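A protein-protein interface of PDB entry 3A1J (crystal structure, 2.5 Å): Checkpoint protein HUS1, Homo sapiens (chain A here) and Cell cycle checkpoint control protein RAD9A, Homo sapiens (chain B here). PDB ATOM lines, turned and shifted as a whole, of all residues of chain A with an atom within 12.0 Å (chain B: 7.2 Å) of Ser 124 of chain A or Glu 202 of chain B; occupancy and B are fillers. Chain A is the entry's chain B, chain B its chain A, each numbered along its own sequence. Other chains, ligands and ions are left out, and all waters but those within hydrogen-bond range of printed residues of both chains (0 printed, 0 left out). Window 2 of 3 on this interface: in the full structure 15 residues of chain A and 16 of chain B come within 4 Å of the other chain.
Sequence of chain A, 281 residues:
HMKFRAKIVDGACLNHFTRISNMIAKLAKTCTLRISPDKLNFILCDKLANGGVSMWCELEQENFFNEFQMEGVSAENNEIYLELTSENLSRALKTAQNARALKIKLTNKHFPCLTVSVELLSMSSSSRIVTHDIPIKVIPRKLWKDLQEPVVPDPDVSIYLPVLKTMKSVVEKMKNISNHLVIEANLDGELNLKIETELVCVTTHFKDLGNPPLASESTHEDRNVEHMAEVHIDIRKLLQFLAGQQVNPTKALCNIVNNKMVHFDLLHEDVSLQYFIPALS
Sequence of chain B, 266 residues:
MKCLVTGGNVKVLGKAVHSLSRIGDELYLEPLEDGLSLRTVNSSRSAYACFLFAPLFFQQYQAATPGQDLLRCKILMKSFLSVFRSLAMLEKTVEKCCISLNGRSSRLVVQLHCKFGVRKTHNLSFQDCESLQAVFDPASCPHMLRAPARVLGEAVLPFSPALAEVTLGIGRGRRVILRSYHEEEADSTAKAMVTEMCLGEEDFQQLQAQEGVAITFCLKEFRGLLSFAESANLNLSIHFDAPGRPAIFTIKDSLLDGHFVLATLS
Hydrophobic or aromatic side chains of chain B within 4 Å of the printed part of chain A: Val 151 and Leu 199.
Of the 14 printed residues of chain A, 4 touch a printed residue of chain B.
Printed residues of chain A that touch a printed residue of chain B: Ser 124, Ser 126, Ser 127 and Arg 128.
Among the printed residues, 7 pairs touch across the chains.
The guanidinium group of Arg 175 of chain B sits at hydrogen-bond distance from the backbone carbonyl oxygen of Ser 127 of chain A, 3.3 Å away.
OE1 of Glu 202 of chain B is in hydrogen-bond range of OG of Ser 124 of chain A (3.2 Å).
The side-chain carboxylate of Glu 202 of chain B lies within hydrogen-bond range of the side-chain hydroxyl of Ser 126 of chain A, 3.0 Å away.
The side-chain carboxylate of Asp 203 of chain B lies within salt-bridge range of the guanidinium group of Arg 128 of chain A (2.8 Å).
N of Gly 200 of chain B is in hydrogen-bond range of OD2 of Asp 203 of chain B (3.4 Å).
N of Leu 120 of chain A is in hydrogen-bond range of O of Arg 128 of chain A, at 2.9 Å.
OG of Ser 122 of chain A lies within hydrogen-bond range of OG of Ser 124 of chain A (3.0 Å).
The side-chain hydroxyl (OG) of Ser 122 of chain A sits at hydrogen-bond distance from the backbone carbonyl oxygen (O) of Ser 126 of chain A, 3.4 Å away.
The backbone carbonyl oxygen (O) of Ser 126 of chain A sits at hydrogen-bond distance from the side-chain hydroxyl (OG) of Ser 124 of chain A (3.2 Å).
Ser 124 of chain A touches just one residue of chain B: Glu 202.
Glu 202 of chain B touches just these residues of chain A: Ser 124 and Ser 126.
No residue of chain A comes within 4 Å of Gly 200 of chain B.
No residue of chain A comes within 4 Å of Glu 201 of chain B.
Printed residues of chain A within 4 Å of Val 151 of chain B: Arg 128.
Of the printed residues of chain B, Ser 127 of chain A touches Arg 175.
Of the printed residues of chain B, Ser 126 of chain A touches Arg 175 (3.5 Å) and Glu 202 (3.0 Å).
Of the printed residues of chain A, Leu 199 of chain B touches Arg 128.
Leu 121 of chain A touches none of the printed residues of chain B.
Among the printed residues, pairs that only touch across the chains: Ser 126 of chain A with Arg 175 of chain B (3.5 Å), Arg 128 of chain A with Val 151 of chain B (3.6 Å) and Arg 128 of chain A with Leu 199 of chain B (3.5 Å).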
ATOM      1  N   ASN A  98     -16.628   4.943 -29.680  1.00  0.00           N
ATOM      2  CA  ASN A  98     -16.022   4.335 -28.505  1.00  0.00           C
ATOM      3  C   ASN A  98     -15.633   5.444 -27.553  1.00  0.00           C
ATOM      4  O   ASN A  98     -14.577   5.386 -26.926  1.00  0.00           O
ATOM      5  CB  ASN A  98     -14.767   3.550 -28.899  1.00  0.00           C
ATOM      6  CG  ASN A  98     -15.058   2.444 -29.900  1.00  0.00           C
ATOM      7  OD1 ASN A  98     -15.777   1.487 -29.597  1.00  0.00           O
ATOM      8  ND2 ASN A  98     -14.500   2.570 -31.101  1.00  0.00           N
ATOM      9  N   ARG A 100     -16.243   8.070 -24.228  1.00  0.00           N
ATOM     10  CA  ARG A 100     -16.813   8.151 -22.894  1.00  0.00           C
ATOM     11  C   ARG A 100     -17.410   9.540 -22.782  1.00  0.00           C
ATOM     12  O   ARG A 100     -18.519   9.715 -22.278  1.00  0.00           O
ATOM     13  CB  ARG A 100     -15.722   7.980 -21.844  1.00  0.00           C
ATOM     14  CG  ARG A 100     -16.200   8.093 -20.415  1.00  0.00           C
ATOM     15  CD  ARG A 100     -15.056   7.752 -19.474  1.00  0.00           C
ATOM     16  NE  ARG A 100     -15.456   7.674 -18.070  1.00  0.00           N
ATOM     17  CZ  ARG A 100     -14.665   7.230 -17.096  1.00  0.00           C
ATOM     18  NH1 ARG A 100     -13.429   6.822 -17.373  1.00  0.00           N
ATOM     19  NH2 ARG A 100     -15.109   7.192 -15.846  1.00  0.00           N
ATOM     20  N   ALA A 101     -16.663  10.530 -23.267  1.00  0.00           N
ATOM     21  CA  ALA A 101     -17.115  11.913 -23.226  1.00  0.00           C
ATOM     22  C   ALA A 101     -16.591  12.747 -24.393  1.00  0.00           C
ATOM     23  O   ALA A 101     -15.629  12.383 -25.063  1.00  0.00           O
ATOM     24  CB  ALA A 101     -16.703  12.554 -21.906  1.00  0.00           C
ATOM     25  N   GLU A 119     -12.692  11.844 -25.283  1.00  0.00           N
ATOM     26  CA  GLU A 119     -12.095  11.009 -24.246  1.00  0.00           C
ATOM     27  C   GLU A 119     -12.577   9.592 -24.522  1.00  0.00           C
ATOM     28  O   GLU A 119     -13.747   9.276 -24.307  1.00  0.00           O
ATOM     29  CB  GLU A 119     -12.564  11.472 -22.867  1.00  0.00           C
ATOM     30  CG  GLU A 119     -11.929  10.758 -21.689  1.00  0.00           C
ATOM     31  CD  GLU A 119     -12.634  11.071 -20.370  1.00  0.00           C
ATOM     32  OE1 GLU A 119     -12.711  12.263 -19.986  1.00  0.00           O
ATOM     33  OE2 GLU A 119     -13.117  10.116 -19.718  1.00  0.00           O
ATOM     34  N   LEU A 120     -11.680   8.746 -25.016  1.00  0.00           N
ATOM     35  CA  LEU A 120     -12.034   7.371 -25.351  1.00  0.00           C
ATOM     36  C   LEU A 120     -12.320   6.498 -24.133  1.00  0.00           C
ATOM     37  O   LEU A 120     -11.819   6.744 -23.035  1.00  0.00           O
ATOM     38  CB  LEU A 120     -10.929   6.727 -26.197  1.00  0.00           C
ATOM     39  CG  LEU A 120     -10.536   7.459 -27.488  1.00  0.00           C
ATOM     40  CD1 LEU A 120      -9.470   6.656 -28.229  1.00  0.00           C
ATOM     41  CD2 LEU A 120     -11.759   7.659 -28.373  1.00  0.00           C
ATOM     42  N   LEU A 121     -13.144   5.479 -24.351  1.00  0.00           N
ATOM     43  CA  LEU A 121     -13.528   4.537 -23.319  1.00  0.00           C
ATOM     44  C   LEU A 121     -12.260   3.896 -22.793  1.00  0.00           C
ATOM     45  O   LEU A 121     -11.344   3.603 -23.553  1.00  0.00           O
ATOM     46  CB  LEU A 121     -14.450   3.470 -23.919  1.00  0.00           C
ATOM     47  CG  LEU A 121     -15.959   3.433 -23.605  1.00  0.00           C
ATOM     48  CD1 LEU A 121     -16.502   4.805 -23.206  1.00  0.00           C
ATOM     49  CD2 LEU A 121     -16.692   2.887 -24.831  1.00  0.00           C
ATOM     50  N   SER A 122     -12.202   3.689 -21.488  1.00  0.00           N
ATOM     51  CA  SER A 122     -11.034   3.074 -20.881  1.00  0.00           C
ATOM     52  C   SER A 122     -11.429   2.272 -19.650  1.00  0.00           C
ATOM     53  O   SER A 122     -12.483   2.511 -19.046  1.00  0.00           O
ATOM     54  CB  SER A 122     -10.013   4.142 -20.493  1.00  0.00           C
ATOM     55  OG  SER A 122      -8.959   3.572 -19.741  1.00  0.00           O
ATOM     56  N   MET A 123     -10.578   1.319 -19.285  1.00  0.00           N
ATOM     57  CA  MET A 123     -10.823   0.471 -18.125  1.00  0.00           C
ATOM     58  C   MET A 123     -10.016   0.944 -16.916  1.00  0.00           C
ATOM     59  O   MET A 123     -10.251   0.509 -15.784  1.00  0.00           O
ATOM     60  CB  MET A 123     -10.480  -0.980 -18.471  1.00  0.00           C
ATOM     61  CG  MET A 123     -11.514  -1.645 -19.377  1.00  0.00           C
ATOM     62  SD  MET A 123     -13.295  -1.569 -18.581  1.00  0.00           S
ATOM     63  CE  MET A 123     -13.083  -2.970 -17.273  1.00  0.00           C
ATOM     64  N   SER A 124      -9.083   1.860 -17.171  1.00  0.00           N
ATOM     65  CA  SER A 124      -8.213   2.425 -16.143  1.00  0.00           C
ATOM     66  C   SER A 124      -8.588   3.867 -15.792  1.00  0.00           C
ATOM     67  O   SER A 124      -9.633   4.367 -16.207  1.00  0.00           O
ATOM     68  CB  SER A 124      -6.764   2.375 -16.628  1.00  0.00           C
ATOM     69  OG  SER A 124      -6.651   2.934 -17.925  1.00  0.00           O
ATOM     70  N   SER A 125      -7.729   4.531 -15.022  1.00  0.00           N
ATOM     71  CA  SER A 125      -7.971   5.917 -14.625  1.00  0.00           C
ATOM     72  C   SER A 125      -7.555   6.877 -15.731  1.00  0.00           C
ATOM     73  O   SER A 125      -8.032   8.009 -15.788  1.00  0.00           O
ATOM     74  CB  SER A 125      -7.185   6.262 -13.361  1.00  0.00           C
ATOM     75  OG  SER A 125      -7.582   5.449 -12.279  1.00  0.00           O
ATOM     76  N   SER A 126      -6.666   6.424 -16.606  1.00  0.00           N
ATOM     77  CA  SER A 126      -6.190   7.261 -17.698  1.00  0.00           C
ATOM     78  C   SER A 126      -6.711   6.780 -19.042  1.00  0.00           C
ATOM     79  O   SER A 126      -6.324   5.719 -19.527  1.00  0.00           O
ATOM     80  CB  SER A 126      -4.661   7.268 -17.727  1.00  0.00           C
ATOM     81  OG  SER A 126      -4.164   5.966 -17.994  1.00  0.00           O
ATOM     82  N   SER A 127      -7.586   7.569 -19.648  1.00  0.00           N
ATOM     83  CA  SER A 127      -8.136   7.213 -20.943  1.00  0.00           C
ATOM     84  C   SER A 127      -7.379   7.930 -22.059  1.00  0.00           C
ATOM     85  O   SER A 127      -6.759   8.973 -21.837  1.00  0.00           O
ATOM     86  CB  SER A 127      -9.604   7.600 -20.995  1.00  0.00           C
ATOM     87  OG  SER A 127      -9.743   8.973 -20.689  1.00  0.00           O
ATOM     88  N   ARG A 128      -7.424   7.358 -23.258  1.00  0.00           N
ATOM     89  CA  ARG A 128      -6.765   7.963 -24.403  1.00  0.00           C
ATOM     90  C   ARG A 128      -7.609   9.164 -24.797  1.00  0.00           C
ATOM     91  O   ARG A 128      -8.834   9.126 -24.678  1.00  0.00           O
ATOM     92  CB  ARG A 128      -6.694   6.979 -25.570  1.00  0.00           C
ATOM     93  CG  ARG A 128      -5.871   5.738 -25.310  1.00  0.00           C
ATOM     94  CD  ARG A 128      -6.130   4.704 -26.403  1.00  0.00           C
ATOM     95  NE  ARG A 128      -5.459   3.436 -26.134  1.00  0.00           N
ATOM     96  CZ  ARG A 128      -5.562   2.360 -26.906  1.00  0.00           C
ATOM     97  NH1 ARG A 128      -6.310   2.399 -27.996  1.00  0.00           N
ATOM     98  NH2 ARG A 128      -4.914   1.246 -26.587  1.00  0.00           N
ATOM     99  N   ILE A 129      -6.949  10.223 -25.263  1.00  0.00           N
ATOM    100  CA  ILE A 129      -7.631  11.447 -25.653  1.00  0.00           C
ATOM    101  C   ILE A 129      -7.310  11.848 -27.088  1.00  0.00           C
ATOM    102  O   ILE A 129      -6.146  11.944 -27.471  1.00  0.00           O
ATOM    103  CB  ILE A 129      -7.213  12.640 -24.749  1.00  0.00           C
ATOM    104  CG1 ILE A 129      -7.280  12.252 -23.271  1.00  0.00           C
ATOM    105  CG2 ILE A 129      -8.117  13.843 -25.028  1.00  0.00           C
ATOM    106  CD1 ILE A 129      -8.673  12.147 -22.728  1.00  0.00           C
ATOM    107  N   VAL B 151      -2.475  -2.149 -31.116  1.00  0.00           N
ATOM    108  CA  VAL B 151      -2.565  -0.931 -30.319  1.00  0.00           C
ATOM    109  C   VAL B 151      -2.134   0.311 -31.105  1.00  0.00           C
ATOM    110  O   VAL B 151      -2.814   1.335 -31.077  1.00  0.00           O
ATOM    111  CB  VAL B 151      -1.726  -1.058 -29.036  1.00  0.00           C
ATOM    112  CG1 VAL B 151      -1.839   0.209 -28.205  1.00  0.00           C
ATOM    113  CG2 VAL B 151      -2.211  -2.260 -28.227  1.00  0.00           C
ATOM    114  N   GLY B 173       4.308  12.137 -17.766  1.00  0.00           N
ATOM    115  CA  GLY B 173       3.459  11.058 -17.292  1.00  0.00           C
ATOM    116  C   GLY B 173       3.661   9.849 -18.176  1.00  0.00           C
ATOM    117  O   GLY B 173       2.940   8.851 -18.080  1.00  0.00           O
ATOM    118  N   ARG B 174       4.662   9.950 -19.043  1.00  0.00           N
ATOM    119  CA  ARG B 174       4.995   8.889 -19.974  1.00  0.00           C
ATOM    120  C   ARG B 174       3.842   8.647 -20.943  1.00  0.00           C
ATOM    121  O   ARG B 174       3.520   7.509 -21.289  1.00  0.00           O
ATOM    122  CB  ARG B 174       5.352   7.614 -19.211  1.00  0.00           C
ATOM    123  CG  ARG B 174       6.383   7.846 -18.117  1.00  0.00           C
ATOM    124  CD  ARG B 174       6.940   6.538 -17.603  1.00  0.00           C
ATOM    125  NE  ARG B 174       7.938   5.994 -18.512  1.00  0.00           N
ATOM    126  CZ  ARG B 174       7.985   4.724 -18.901  1.00  0.00           C
ATOM    127  NH1 ARG B 174       7.081   3.851 -18.470  1.00  0.00           N
ATOM    128  NH2 ARG B 174       8.947   4.324 -19.718  1.00  0.00           N
ATOM    129  N   ARG B 175       3.227   9.746 -21.367  1.00  0.00           N
ATOM    130  CA  ARG B 175       2.130   9.718 -22.319  1.00  0.00           C
ATOM    131  C   ARG B 175       2.793   9.801 -23.691  1.00  0.00           C
ATOM    132  O   ARG B 175       3.735  10.578 -23.873  1.00  0.00           O
ATOM    133  CB  ARG B 175       1.225  10.940 -22.132  1.00  0.00           C
ATOM    134  CG  ARG B 175       0.690  11.156 -20.718  1.00  0.00           C
ATOM    135  CD  ARG B 175      -0.498  10.264 -20.396  1.00  0.00           C
ATOM    136  NE  ARG B 175      -1.587  10.445 -21.356  1.00  0.00           N
ATOM    137  CZ  ARG B 175      -2.846  10.058 -21.151  1.00  0.00           C
ATOM    138  NH1 ARG B 175      -3.188   9.470 -20.010  1.00  0.00           N
ATOM    139  NH2 ARG B 175      -3.760  10.246 -22.094  1.00  0.00           N
ATOM    140  N   LEU B 199      -1.805   8.770 -25.891  1.00  0.00           N
ATOM    141  CA  LEU B 199      -1.969   7.419 -25.368  1.00  0.00           C
ATOM    142  C   LEU B 199      -1.460   7.224 -23.957  1.00  0.00           C
ATOM    143  O   LEU B 199      -0.477   7.848 -23.549  1.00  0.00           O
ATOM    144  CB  LEU B 199      -1.244   6.433 -26.276  1.00  0.00           C
ATOM    145  CG  LEU B 199      -1.773   6.328 -27.698  1.00  0.00           C
ATOM    146  CD1 LEU B 199      -0.698   5.765 -28.601  1.00  0.00           C
ATOM    147  CD2 LEU B 199      -3.014   5.456 -27.704  1.00  0.00           C
ATOM    148  N   GLY B 200      -2.120   6.333 -23.220  1.00  0.00           N
ATOM    149  CA  GLY B 200      -1.702   6.050 -21.859  1.00  0.00           C
ATOM    150  C   GLY B 200      -0.362   5.329 -21.855  1.00  0.00           C
ATOM    151  O   GLY B 200       0.065   4.793 -22.879  1.00  0.00           O
ATOM    152  N   GLU B 201       0.309   5.317 -20.710  1.00  0.00           N
ATOM    153  CA  GLU B 201       1.603   4.656 -20.591  1.00  0.00           C
ATOM    154  C   GLU B 201       1.405   3.147 -20.583  1.00  0.00           C
ATOM    155  O   GLU B 201       2.271   2.394 -21.027  1.00  0.00           O
ATOM    156  CB  GLU B 201       2.291   5.080 -19.295  1.00  0.00           C
ATOM    157  CG  GLU B 201       3.730   4.610 -19.171  1.00  0.00           C
ATOM    158  CD  GLU B 201       4.253   4.719 -17.744  1.00  0.00           C
ATOM    159  OE1 GLU B 201       4.046   5.779 -17.109  1.00  0.00           O
ATOM    160  OE2 GLU B 201       4.873   3.747 -17.259  1.00  0.00           O
ATOM    161  N   GLU B 202       0.253   2.717 -20.081  1.00  0.00           N
ATOM    162  CA  GLU B 202      -0.063   1.300 -19.995  1.00  0.00           C
ATOM    163  C   GLU B 202      -0.341   0.661 -21.343  1.00  0.00           C
ATOM    164  O   GLU B 202      -0.523  -0.551 -21.431  1.00  0.00           O
ATOM    165  CB  GLU B 202      -1.253   1.075 -19.053  1.00  0.00           C
ATOM    166  CG  GLU B 202      -1.872   2.348 -18.477  1.00  0.00           C
ATOM    167  CD  GLU B 202      -2.980   2.917 -19.352  1.00  0.00           C
ATOM    168  OE1 GLU B 202      -4.020   2.234 -19.510  1.00  0.00           O
ATOM    169  OE2 GLU B 202      -2.816   4.041 -19.877  1.00  0.00           O
ATOM    170  N   ASP B 203      -0.378   1.467 -22.399  1.00  0.00           N
ATOM    171  CA  ASP B 203      -0.622   0.925 -23.730  1.00  0.00           C
ATOM    172  C   ASP B 203       0.668   0.392 -24.358  1.00  0.00           C
ATOM    173  O   ASP B 203       0.632  -0.285 -25.386  1.00  0.00           O
ATOM    174  CB  ASP B 203      -1.235   1.984 -24.654  1.00  0.00           C
ATOM    175  CG  ASP B 203      -2.721   2.186 -24.414  1.00  0.00           C
ATOM    176  OD1 ASP B 203      -3.439   1.185 -24.186  1.00  0.00           O
ATOM    177  OD2 ASP B 203      -3.175   3.348 -24.476  1.00  0.00           O
ATOM    178  N   PHE B 204       1.804   0.699 -23.739  1.00  0.00           N
ATOM    179  CA  PHE B 204       3.094   0.248 -24.255  1.00  0.00           C
ATOM    180  C   PHE B 204       3.732  -0.834 -23.399  1.00  0.00           C
ATOM    181  O   PHE B 204       3.819  -0.711 -22.182  1.00  0.00           O
ATOM    182  CB  PHE B 204       4.053   1.436 -24.376  1.00  0.00           C
ATOM    183  CG  PHE B 204       3.695   2.386 -25.479  1.00  0.00           C
ATOM    184  CD1 PHE B 204       4.247   2.241 -26.740  1.00  0.00           C
ATOM    185  CD2 PHE B 204       2.757   3.393 -25.271  1.00  0.00           C
ATOM    186  CE1 PHE B 204       3.866   3.087 -27.780  1.00  0.00           C
ATOM    187  CE2 PHE B 204       2.372   4.238 -26.305  1.00  0.00           C
ATOM    188  CZ  PHE B 204       2.925   4.084 -27.556  1.00  0.00           C
ATOM    189  N   GLN B 205       4.174  -1.900 -24.050  1.00  0.00           N
ATOM    190  CA  GLN B 205       4.835  -3.003 -23.361  1.00  0.00           C
ATOM    191  C   GLN B 205       6.193  -2.510 -22.869  1.00  0.00           C
ATOM    192  O   GLN B 205       6.690  -2.950 -21.840  1.00  0.00           O
ATOM    193  CB  GLN B 205       5.016  -4.180 -24.316  1.00  0.00           C
ATOM    194  CG  GLN B 205       3.712  -4.773 -24.835  1.00  0.00           C
ATOM    195  CD  GLN B 205       3.926  -5.634 -26.064  1.00  0.00           C
ATOM    196  OE1 GLN B 205       3.058  -6.414 -26.445  1.00  0.00           O
ATOM    197  NE2 GLN B 205       5.089  -5.491 -26.697  1.00  0.00           N
